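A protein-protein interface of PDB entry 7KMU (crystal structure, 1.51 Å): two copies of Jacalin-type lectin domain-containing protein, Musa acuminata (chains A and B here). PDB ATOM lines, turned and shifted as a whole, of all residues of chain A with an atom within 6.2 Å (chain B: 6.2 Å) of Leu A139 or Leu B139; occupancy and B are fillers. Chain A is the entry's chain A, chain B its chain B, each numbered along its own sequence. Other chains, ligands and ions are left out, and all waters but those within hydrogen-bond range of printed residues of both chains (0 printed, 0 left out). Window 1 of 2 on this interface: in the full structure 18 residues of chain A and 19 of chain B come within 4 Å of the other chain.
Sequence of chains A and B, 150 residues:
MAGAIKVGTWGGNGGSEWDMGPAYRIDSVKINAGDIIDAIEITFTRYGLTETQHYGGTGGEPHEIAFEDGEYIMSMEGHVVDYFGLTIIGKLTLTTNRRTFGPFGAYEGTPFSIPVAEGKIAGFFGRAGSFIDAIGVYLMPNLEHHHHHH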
ATOM      1  N   ALA A   4     -12.048  -1.674 -11.850  1.00  0.00           N
ATOM      2  CA  ALA A   4     -12.125  -2.912 -11.080  1.00  0.00           C
ATOM      3  C   ALA A   4     -10.925  -3.072 -10.142  1.00  0.00           C
ATOM      4  O   ALA A   4      -9.940  -2.328 -10.242  1.00  0.00           O
ATOM      5  CB  ALA A   4     -12.216  -4.110 -12.022  1.00  0.00           C
ATOM      6  N   ILE A   5     -11.036  -4.024  -9.199  1.00  0.00           N
ATOM      7  CA  ILE A   5      -9.950  -4.392  -8.300  1.00  0.00           C
ATOM      8  C   ILE A   5      -9.625  -5.823  -8.651  1.00  0.00           C
ATOM      9  O   ILE A   5     -10.419  -6.724  -8.389  1.00  0.00           O
ATOM     10  CB  ILE A   5     -10.250  -4.171  -6.802  1.00  0.00           C
ATOM     11  CG1 ILE A   5     -10.598  -2.675  -6.572  1.00  0.00           C
ATOM     12  CG2 ILE A   5      -9.031  -4.637  -5.945  1.00  0.00           C
ATOM     13  CD1 ILE A   5     -10.840  -2.234  -5.197  1.00  0.00           C
ATOM     14  N   LYS A   6      -8.479  -6.012  -9.295  1.00  0.00           N
ATOM     15  CA  LYS A   6      -8.018  -7.316  -9.759  1.00  0.00           C
ATOM     16  C   LYS A   6      -6.678  -7.629  -9.120  1.00  0.00           C
ATOM     17  O   LYS A   6      -5.745  -6.827  -9.218  1.00  0.00           O
ATOM     18  CB  LYS A   6      -7.874  -7.312 -11.283  1.00  0.00           C
ATOM     19  CG  LYS A   6      -9.218  -7.302 -12.003  1.00  0.00           C
ATOM     20  CD  LYS A   6      -9.079  -7.171 -13.516  1.00  0.00           C
ATOM     21  CE  LYS A   6      -8.706  -8.468 -14.194  1.00  0.00           C
ATOM     22  NZ  LYS A   6      -8.704  -8.326 -15.681  1.00  0.00           N
ATOM     23  N   VAL A   7      -6.580  -8.782  -8.454  1.00  0.00           N
ATOM     24  CA  VAL A   7      -5.344  -9.214  -7.813  1.00  0.00           C
ATOM     25  C   VAL A   7      -4.917 -10.525  -8.450  1.00  0.00           C
ATOM     26  O   VAL A   7      -5.699 -11.472  -8.549  1.00  0.00           O
ATOM     27  CB  VAL A   7      -5.455  -9.286  -6.269  1.00  0.00           C
ATOM     28  CG1 VAL A   7      -4.150  -9.790  -5.640  1.00  0.00           C
ATOM     29  CG2 VAL A   7      -5.802  -7.916  -5.706  1.00  0.00           C
ATOM     30  N   ILE A 114      -4.585 -15.356  -0.863  1.00  0.00           N
ATOM     31  CA  ILE A 114      -5.264 -14.073  -0.887  1.00  0.00           C
ATOM     32  C   ILE A 114      -6.471 -14.106   0.078  1.00  0.00           C
ATOM     33  O   ILE A 114      -7.629 -14.211  -0.342  1.00  0.00           O
ATOM     34  CB  ILE A 114      -5.570 -13.568  -2.330  1.00  0.00           C
ATOM     35  CG1 ILE A 114      -6.162 -12.146  -2.334  1.00  0.00           C
ATOM     36  CG2 ILE A 114      -6.423 -14.537  -3.166  1.00  0.00           C
ATOM     37  CD1 ILE A 114      -5.097 -11.069  -1.947  1.00  0.00           C
ATOM     38  N   VAL A 116      -9.264 -12.460   2.300  1.00  0.00           N
ATOM     39  CA  VAL A 116      -9.991 -11.199   2.225  1.00  0.00           C
ATOM     40  C   VAL A 116     -10.581 -10.921   3.606  1.00  0.00           C
ATOM     41  O   VAL A 116     -11.496 -11.633   4.042  1.00  0.00           O
ATOM     42  CB  VAL A 116     -11.072 -11.207   1.102  1.00  0.00           C
ATOM     43  CG1 VAL A 116     -11.662  -9.811   0.915  1.00  0.00           C
ATOM     44  CG2 VAL A 116     -10.500 -11.709  -0.228  1.00  0.00           C
ATOM     45  N   LYS A 120     -15.131  -9.380  -0.649  1.00  0.00           N
ATOM     46  CA  LYS A 120     -15.271 -10.741  -1.161  1.00  0.00           C
ATOM     47  C   LYS A 120     -14.554 -10.948  -2.475  1.00  0.00           C
ATOM     48  O   LYS A 120     -14.320  -9.996  -3.222  1.00  0.00           O
ATOM     49  CB  LYS A 120     -16.777 -11.069  -1.351  1.00  0.00           C
ATOM     50  CG  LYS A 120     -17.498 -10.182  -2.371  1.00  0.00           C
ATOM     51  CD  LYS A 120     -18.951 -10.618  -2.569  1.00  0.00           C
ATOM     52  CE  LYS A 120     -19.648  -9.742  -3.576  1.00  0.00           C
ATOM     53  NZ  LYS A 120     -20.970 -10.307  -3.965  1.00  0.00           N
ATOM     54  N   ILE A 121     -14.258 -12.215  -2.787  1.00  0.00           N
ATOM     55  CA  ILE A 121     -13.777 -12.608  -4.102  1.00  0.00           C
ATOM     56  C   ILE A 121     -15.056 -12.752  -4.943  1.00  0.00           C
ATOM     57  O   ILE A 121     -15.937 -13.572  -4.621  1.00  0.00           O
ATOM     58  CB  ILE A 121     -12.948 -13.900  -4.038  1.00  0.00           C
ATOM     59  CG1 ILE A 121     -11.548 -13.589  -3.495  1.00  0.00           C
ATOM     60  CG2 ILE A 121     -12.880 -14.584  -5.421  1.00  0.00           C
ATOM     61  CD1 ILE A 121     -10.789 -14.798  -2.914  1.00  0.00           C
ATOM     62  N   ALA A 122     -15.182 -11.910  -5.979  1.00  0.00           N
ATOM     63  CA  ALA A 122     -16.391 -11.865  -6.792  1.00  0.00           C
ATOM     64  C   ALA A 122     -16.271 -12.461  -8.178  1.00  0.00           C
ATOM     65  O   ALA A 122     -17.239 -12.446  -8.938  1.00  0.00           O
ATOM     66  CB  ALA A 122     -16.879 -10.436  -6.890  1.00  0.00           C
ATOM     67  N   GLY A 123     -15.110 -13.003  -8.503  1.00  0.00           N
ATOM     68  CA  GLY A 123     -14.898 -13.572  -9.822  1.00  0.00           C
ATOM     69  C   GLY A 123     -13.442 -13.895 -10.021  1.00  0.00           C
ATOM     70  O   GLY A 123     -12.608 -13.631  -9.140  1.00  0.00           O
ATOM     71  N   VAL A 137      -8.038 -12.997  -8.972  1.00  0.00           N
ATOM     72  CA  VAL A 137      -9.389 -12.708  -8.480  1.00  0.00           C
ATOM     73  C   VAL A 137      -9.826 -11.273  -8.641  1.00  0.00           C
ATOM     74  O   VAL A 137      -9.009 -10.347  -8.550  1.00  0.00           O
ATOM     75  CB  VAL A 137      -9.539 -13.116  -6.978  1.00  0.00           C
ATOM     76  CG1 VAL A 137      -9.488 -14.635  -6.799  1.00  0.00           C
ATOM     77  CG2 VAL A 137      -8.505 -12.421  -6.078  1.00  0.00           C
ATOM     78  N   TYR A 138     -11.143 -11.097  -8.795  1.00  0.00           N
ATOM     79  CA  TYR A 138     -11.800  -9.798  -8.713  1.00  0.00           C
ATOM     80  C   TYR A 138     -12.214  -9.646  -7.257  1.00  0.00           C
ATOM     81  O   TYR A 138     -12.725 -10.602  -6.657  1.00  0.00           O
ATOM     82  CB  TYR A 138     -13.081  -9.765  -9.551  1.00  0.00           C
ATOM     83  CG  TYR A 138     -12.810  -9.538 -11.014  1.00  0.00           C
ATOM     84  CD1 TYR A 138     -12.543 -10.604 -11.862  1.00  0.00           C
ATOM     85  CD2 TYR A 138     -12.817  -8.253 -11.554  1.00  0.00           C
ATOM     86  CE1 TYR A 138     -12.284 -10.402 -13.216  1.00  0.00           C
ATOM     87  CE2 TYR A 138     -12.556  -8.037 -12.903  1.00  0.00           C
ATOM     88  CZ  TYR A 138     -12.313  -9.115 -13.737  1.00  0.00           C
ATOM     89  OH  TYR A 138     -12.070  -8.887 -15.067  1.00  0.00           O
ATOM     90  N   LEU A 139     -12.023  -8.451  -6.695  1.00  0.00           N
ATOM     91  CA  LEU A 139     -12.428  -8.162  -5.329  1.00  0.00           C
ATOM     92  C   LEU A 139     -13.506  -7.102  -5.347  1.00  0.00           C
ATOM     93  O   LEU A 139     -13.425  -6.138  -6.117  1.00  0.00           O
ATOM     94  CB  LEU A 139     -11.251  -7.727  -4.443  1.00  0.00           C
ATOM     95  CG  LEU A 139     -10.121  -8.754  -4.302  1.00  0.00           C
ATOM     96  CD1 LEU A 139      -9.058  -8.218  -3.436  1.00  0.00           C
ATOM     97  CD2 LEU A 139     -10.613 -10.060  -3.689  1.00  0.00           C
ATOM     98  N   MET A 140     -14.534  -7.292  -4.521  1.00  0.00           N
ATOM     99  CA  MET A 140     -15.639  -6.342  -4.431  1.00  0.00           C
ATOM    100  C   MET A 140     -16.000  -6.110  -2.978  1.00  0.00           C
ATOM    101  O   MET A 140     -15.735  -6.981  -2.135  1.00  0.00           O
ATOM    102  CB  MET A 140     -16.858  -6.856  -5.225  1.00  0.00           C
ATOM    103  CG  MET A 140     -16.701  -6.682  -6.713  1.00  0.00           C
ATOM    104  SD  MET A 140     -18.200  -7.040  -7.640  1.00  0.00           S
ATOM    105  CE  MET A 140     -19.035  -5.462  -7.521  1.00  0.00           C
ATOM    106  N   PRO A 141     -16.618  -4.952  -2.623  1.00  0.00           N
ATOM    107  CA  PRO A 141     -17.000  -4.779  -1.221  1.00  0.00           C
ATOM    108  C   PRO A 141     -18.147  -5.724  -0.885  1.00  0.00           C
ATOM    109  O   PRO A 141     -18.834  -6.215  -1.790  1.00  0.00           O
ATOM    110  CB  PRO A 141     -17.455  -3.311  -1.131  1.00  0.00           C
ATOM    111  CG  PRO A 141     -17.707  -2.883  -2.496  1.00  0.00           C
ATOM    112  CD  PRO A 141     -17.018  -3.793  -3.455  1.00  0.00           C
ATOM    113  N   ALA B   4     -14.918  -0.808   2.351  1.00  0.00           N
ATOM    114  CA  ALA B   4     -13.468  -1.031   2.170  1.00  0.00           C
ATOM    115  C   ALA B   4     -13.170  -2.439   1.677  1.00  0.00           C
ATOM    116  O   ALA B   4     -13.967  -3.366   1.861  1.00  0.00           O
ATOM    117  CB  ALA B   4     -12.721  -0.791   3.477  1.00  0.00           C
ATOM    118  N   ILE B   5     -12.002  -2.594   1.035  1.00  0.00           N
ATOM    119  CA  ILE B   5     -11.510  -3.894   0.593  1.00  0.00           C
ATOM    120  C   ILE B   5     -10.171  -4.082   1.301  1.00  0.00           C
ATOM    121  O   ILE B   5      -9.234  -3.297   1.091  1.00  0.00           O
ATOM    122  CB  ILE B   5     -11.386  -4.025  -0.950  1.00  0.00           C
ATOM    123  CG1 ILE B   5     -12.787  -3.966  -1.606  1.00  0.00           C
ATOM    124  CG2 ILE B   5     -10.643  -5.335  -1.294  1.00  0.00           C
ATOM    125  CD1 ILE B   5     -12.823  -3.975  -3.098  1.00  0.00           C
ATOM    126  N   LYS B   6     -10.097  -5.092   2.172  1.00  0.00           N
ATOM    127  CA  LYS B   6      -8.898  -5.403   2.949  1.00  0.00           C
ATOM    128  C   LYS B   6      -8.458  -6.811   2.662  1.00  0.00           C
ATOM    129  O   LYS B   6      -9.260  -7.731   2.780  1.00  0.00           O
ATOM    130  CB  LYS B   6      -9.166  -5.265   4.453  1.00  0.00           C
ATOM    131  CG  LYS B   6      -9.366  -3.810   4.886  1.00  0.00           C
ATOM    132  CD  LYS B   6      -9.858  -3.709   6.331  1.00  0.00           C
ATOM    133  CE  LYS B   6      -8.766  -3.991   7.345  1.00  0.00           C
ATOM    134  NZ  LYS B   6      -9.270  -3.876   8.758  1.00  0.00           N
ATOM    135  N   VAL B   7      -7.185  -6.981   2.266  1.00  0.00           N
ATOM    136  CA  VAL B   7      -6.619  -8.303   2.001  1.00  0.00           C
ATOM    137  C   VAL B   7      -5.480  -8.560   2.962  1.00  0.00           C
ATOM    138  O   VAL B   7      -4.674  -7.673   3.236  1.00  0.00           O
ATOM    139  CB  VAL B   7      -6.255  -8.570   0.524  1.00  0.00           C
ATOM    140  CG1 VAL B   7      -7.498  -8.516  -0.355  1.00  0.00           C
ATOM    141  CG2 VAL B   7      -5.191  -7.594   0.006  1.00  0.00           C
ATOM    142  N   ILE B 114       1.060  -9.993  -3.464  1.00  0.00           N
ATOM    143  CA  ILE B 114      -0.189  -9.322  -3.818  1.00  0.00           C
ATOM    144  C   ILE B 114       0.043  -8.476  -5.058  1.00  0.00           C
ATOM    145  O   ILE B 114       0.273  -7.274  -4.941  1.00  0.00           O
ATOM    146  CB  ILE B 114      -0.779  -8.483  -2.647  1.00  0.00           C
ATOM    147  CG1 ILE B 114      -0.910  -9.310  -1.381  1.00  0.00           C
ATOM    148  CG2 ILE B 114      -2.141  -7.847  -3.022  1.00  0.00           C
ATOM    149  CD1 ILE B 114       0.450  -9.538  -0.552  1.00  0.00           C
ATOM    150  N   VAL B 116      -1.221  -6.303  -7.796  1.00  0.00           N
ATOM    151  CA  VAL B 116      -2.475  -5.629  -8.122  1.00  0.00           C
ATOM    152  C   VAL B 116      -2.490  -5.355  -9.629  1.00  0.00           C
ATOM    153  O   VAL B 116      -1.790  -4.451 -10.108  1.00  0.00           O
ATOM    154  CB  VAL B 116      -2.736  -4.351  -7.270  1.00  0.00           C
ATOM    155  CG1 VAL B 116      -4.124  -3.792  -7.548  1.00  0.00           C
ATOM    156  CG2 VAL B 116      -2.576  -4.639  -5.773  1.00  0.00           C
ATOM    157  N   LYS B 120      -4.993  -0.132  -6.772  1.00  0.00           N
ATOM    158  CA  LYS B 120      -3.829   0.250  -5.978  1.00  0.00           C
ATOM    159  C   LYS B 120      -3.934  -0.147  -4.515  1.00  0.00           C
ATOM    160  O   LYS B 120      -5.034  -0.349  -3.993  1.00  0.00           O
ATOM    161  CB  LYS B 120      -3.576   1.771  -6.086  1.00  0.00           C
ATOM    162  CG  LYS B 120      -4.694   2.643  -5.506  1.00  0.00           C
ATOM    163  CD  LYS B 120      -4.350   4.141  -5.573  1.00  0.00           C
ATOM    164  CE  LYS B 120      -5.549   4.956  -5.141  1.00  0.00           C
ATOM    165  NZ  LYS B 120      -5.313   6.418  -5.275  1.00  0.00           N
ATOM    166  N   ILE B 121      -2.781  -0.228  -3.855  1.00  0.00           N
ATOM    167  CA  ILE B 121      -2.713  -0.427  -2.419  1.00  0.00           C
ATOM    168  C   ILE B 121      -2.837   0.974  -1.811  1.00  0.00           C
ATOM    169  O   ILE B 121      -2.061   1.884  -2.153  1.00  0.00           O
ATOM    170  CB  ILE B 121      -1.410  -1.160  -2.035  1.00  0.00           C
ATOM    171  CG1 ILE B 121      -1.571  -2.655  -2.346  1.00  0.00           C
ATOM    172  CG2 ILE B 121      -1.032  -0.930  -0.539  1.00  0.00           C
ATOM    173  CD1 ILE B 121      -0.288  -3.488  -2.385  1.00  0.00           C
ATOM    174  N   ALA B 122      -3.799   1.143  -0.892  1.00  0.00           N
ATOM    175  CA  ALA B 122      -4.110   2.450  -0.331  1.00  0.00           C
ATOM    176  C   ALA B 122      -3.971   2.566   1.172  1.00  0.00           C
ATOM    177  O   ALA B 122      -4.374   3.575   1.753  1.00  0.00           O
ATOM    178  CB  ALA B 122      -5.526   2.834  -0.738  1.00  0.00           C
ATOM    179  N   GLY B 123      -3.393   1.564   1.806  1.00  0.00           N
ATOM    180  CA  GLY B 123      -3.251   1.579   3.253  1.00  0.00           C
ATOM    181  C   GLY B 123      -2.840   0.223   3.765  1.00  0.00           C
ATOM    182  O   GLY B 123      -2.763  -0.743   3.000  1.00  0.00           O
ATOM    183  N   VAL B 137      -3.210  -5.208   3.453  1.00  0.00           N
ATOM    184  CA  VAL B 137      -3.397  -3.960   2.724  1.00  0.00           C
ATOM    185  C   VAL B 137      -4.838  -3.633   2.403  1.00  0.00           C
ATOM    186  O   VAL B 137      -5.661  -4.535   2.252  1.00  0.00           O
ATOM    187  CB  VAL B 137      -2.546  -3.915   1.421  1.00  0.00           C
ATOM    188  CG1 VAL B 137      -1.047  -3.833   1.732  1.00  0.00           C
ATOM    189  CG2 VAL B 137      -2.849  -5.094   0.495  1.00  0.00           C
ATOM    190  N   TYR B 138      -5.121  -2.327   2.259  1.00  0.00           N
ATOM    191  CA  TYR B 138      -6.385  -1.831   1.732  1.00  0.00           C
ATOM    192  C   TYR B 138      -6.204  -1.692   0.223  1.00  0.00           C
ATOM    193  O   TYR B 138      -5.123  -1.295  -0.242  1.00  0.00           O
ATOM    194  CB  TYR B 138      -6.684  -0.435   2.287  1.00  0.00           C
ATOM    195  CG  TYR B 138      -7.222  -0.466   3.694  1.00  0.00           C
ATOM    196  CD1 TYR B 138      -6.368  -0.571   4.787  1.00  0.00           C
ATOM    197  CD2 TYR B 138      -8.591  -0.419   3.936  1.00  0.00           C
ATOM    198  CE1 TYR B 138      -6.858  -0.583   6.089  1.00  0.00           C
ATOM    199  CE2 TYR B 138      -9.096  -0.429   5.234  1.00  0.00           C
ATOM    200  CZ  TYR B 138      -8.229  -0.521   6.307  1.00  0.00           C
ATOM    201  OH  TYR B 138      -8.752  -0.542   7.574  1.00  0.00           O
ATOM    202  N   LEU B 139      -7.270  -1.970  -0.537  1.00  0.00           N
ATOM    203  CA  LEU B 139      -7.246  -1.846  -1.994  1.00  0.00           C
ATOM    204  C   LEU B 139      -8.303  -0.866  -2.449  1.00  0.00           C
ATOM    205  O   LEU B 139      -9.366  -0.781  -1.842  1.00  0.00           O
ATOM    206  CB  LEU B 139      -7.462  -3.199  -2.693  1.00  0.00           C
ATOM    207  CG  LEU B 139      -6.435  -4.272  -2.338  1.00  0.00           C
ATOM    208  CD1 LEU B 139      -6.796  -5.581  -2.969  1.00  0.00           C
ATOM    209  CD2 LEU B 139      -5.031  -3.881  -2.794  1.00  0.00           C
ATOM    210  N   MET B 140      -8.004  -0.130  -3.523  1.00  0.00           N
ATOM    211  CA  MET B 140      -8.923   0.832  -4.142  1.00  0.00           C
ATOM    212  C   MET B 140      -8.736   0.767  -5.640  1.00  0.00           C
ATOM    213  O   MET B 140      -7.644   0.423  -6.091  1.00  0.00           O
ATOM    214  CB  MET B 140      -8.561   2.257  -3.715  1.00  0.00           C
ATOM    215  CG  MET B 140      -8.917   2.551  -2.343  1.00  0.00           C
ATOM    216  SD  MET B 140      -8.609   4.286  -2.062  1.00  0.00           S
ATOM    217  CE  MET B 140      -9.000   4.312  -0.477  1.00  0.00           C
ATOM    218  N   PRO B 141      -9.737   1.142  -6.463  1.00  0.00           N
ATOM    219  CA  PRO B 141      -9.468   1.210  -7.905  1.00  0.00           C
ATOM    220  C   PRO B 141      -8.639   2.453  -8.230  1.00  0.00           C
ATOM    221  O   PRO B 141      -8.455   3.333  -7.379  1.00  0.00           O
ATOM    222  CB  PRO B 141     -10.868   1.282  -8.535  1.00  0.00           C
ATOM    223  CG  PRO B 141     -11.773   1.721  -7.460  1.00  0.00           C
ATOM    224  CD  PRO B 141     -11.091   1.628  -6.132  1.00  0.00           C
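O of Ile B5 is in hydrogen-bond range of N of Leu B139, 2.9 Å away.
O of Ile A5 is in hydrogen-bond range of N of Leu A139 (2.9 Å).
The backbone NH (N) of Lys B120 is in hydrogen-bond range of the backbone carbonyl oxygen (O) of Met B140 (2.8 Å).
The backbone NH (N) of Val A137 lies within hydrogen-bond range of the backbone carbonyl oxygen (O) of Val A7, at 2.8 Å.
N of Lys A120 sits at hydrogen-bond distance from O of Met A140.
The backbone carbonyl oxygen of Val B7 lies within hydrogen-bond range of the backbone NH of Val B137, 2.9 Å away.
Among the printed residues, merely in contact across the chains: Ile A5 with Ile B5 (3.4 Å), Ile A5 with Leu B139 (3.8 Å), Ile A5 with Met B140 (3.7 Å), Ile A5 with Pro B141 (3.8 Å), Lys A6 with Val B116 (3.6 Å), Val A7 with Ile B114 (3.8 Å), Val A7 with Leu B139 (3.7 Å), Ile A114 with Val B7 (3.7 Å), Val A116 with Lys B6 (3.6 Å), Leu A139 with Ile B5 (3.8 Å), Leu A139 with Val B7 (3.5 Å), Leu A139 with Leu B139 (3.5 Å), Met A140 with Ile B5 (3.8 Å) and Pro A141 with Ile B5 (3.9 Å).
Of the printed residues of chain B, Ile A5 touches Ile B5, Leu B139, Met B140 and Pro B141.
Leu A139 touches three residues of chain B.
Printed residues of chain B within 4 Å of Pro A141: Ile B5.
Of the printed residues of chain A, Ile B5 touches Ile A5 (3.4 Å), Leu A139 (3.8 Å), Met A140 (3.8 Å) and Pro A141 (3.9 Å).
Leu B139 touches just these residues of chain A: Ile A5, Val A7 and Leu A139.
The nearest printed residue of chain B that does not touch Leu A139 is Lys B6 (6.2 Å).
The nearest residue of chain A that does not touch Leu B139 is Ile A114 (5.8 Å).
Hydrophobic or aromatic side chains of chain B that line the printed part of chain A: Ile B5, Val B7, Ile B114, Val B116, Leu B139 and Pro B141.
Of the 15 printed residues of chain A, 8 touch a printed residue of chain B.
Printed residues of chain A that touch a printed residue of chain B: Ile A5, Lys A6, Val A7, Ile A114, Val A116, Leu A139, Met A140 and Pro A141.
Hydrophobic or aromatic side chains of chain A within 4 Å of the printed part of chain B: Ile A5, Val A7, Ile A114, Val A116 and Leu A139.
Ile A5 touches Leu B139, and with the chains exchanged Leu A139 touches Ile B5.
Ile A5 touches Met B140, and with the chains exchanged Met A140 touches Ile B5.
Val A7 touches Leu B139, and with the chains exchanged Leu A139 touches Val B7.
Leu A139 touches its own counterpart, Leu B139.
Positions printed for both chains: 4, 5, 6, 7, 114, 116, 120, 121, 122, 123, 137, 138, 139, 140 and 141.
Of the 14 pairs that touch across the chains among the printed residues, 14 have their exchanged pair printed and touching as well.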
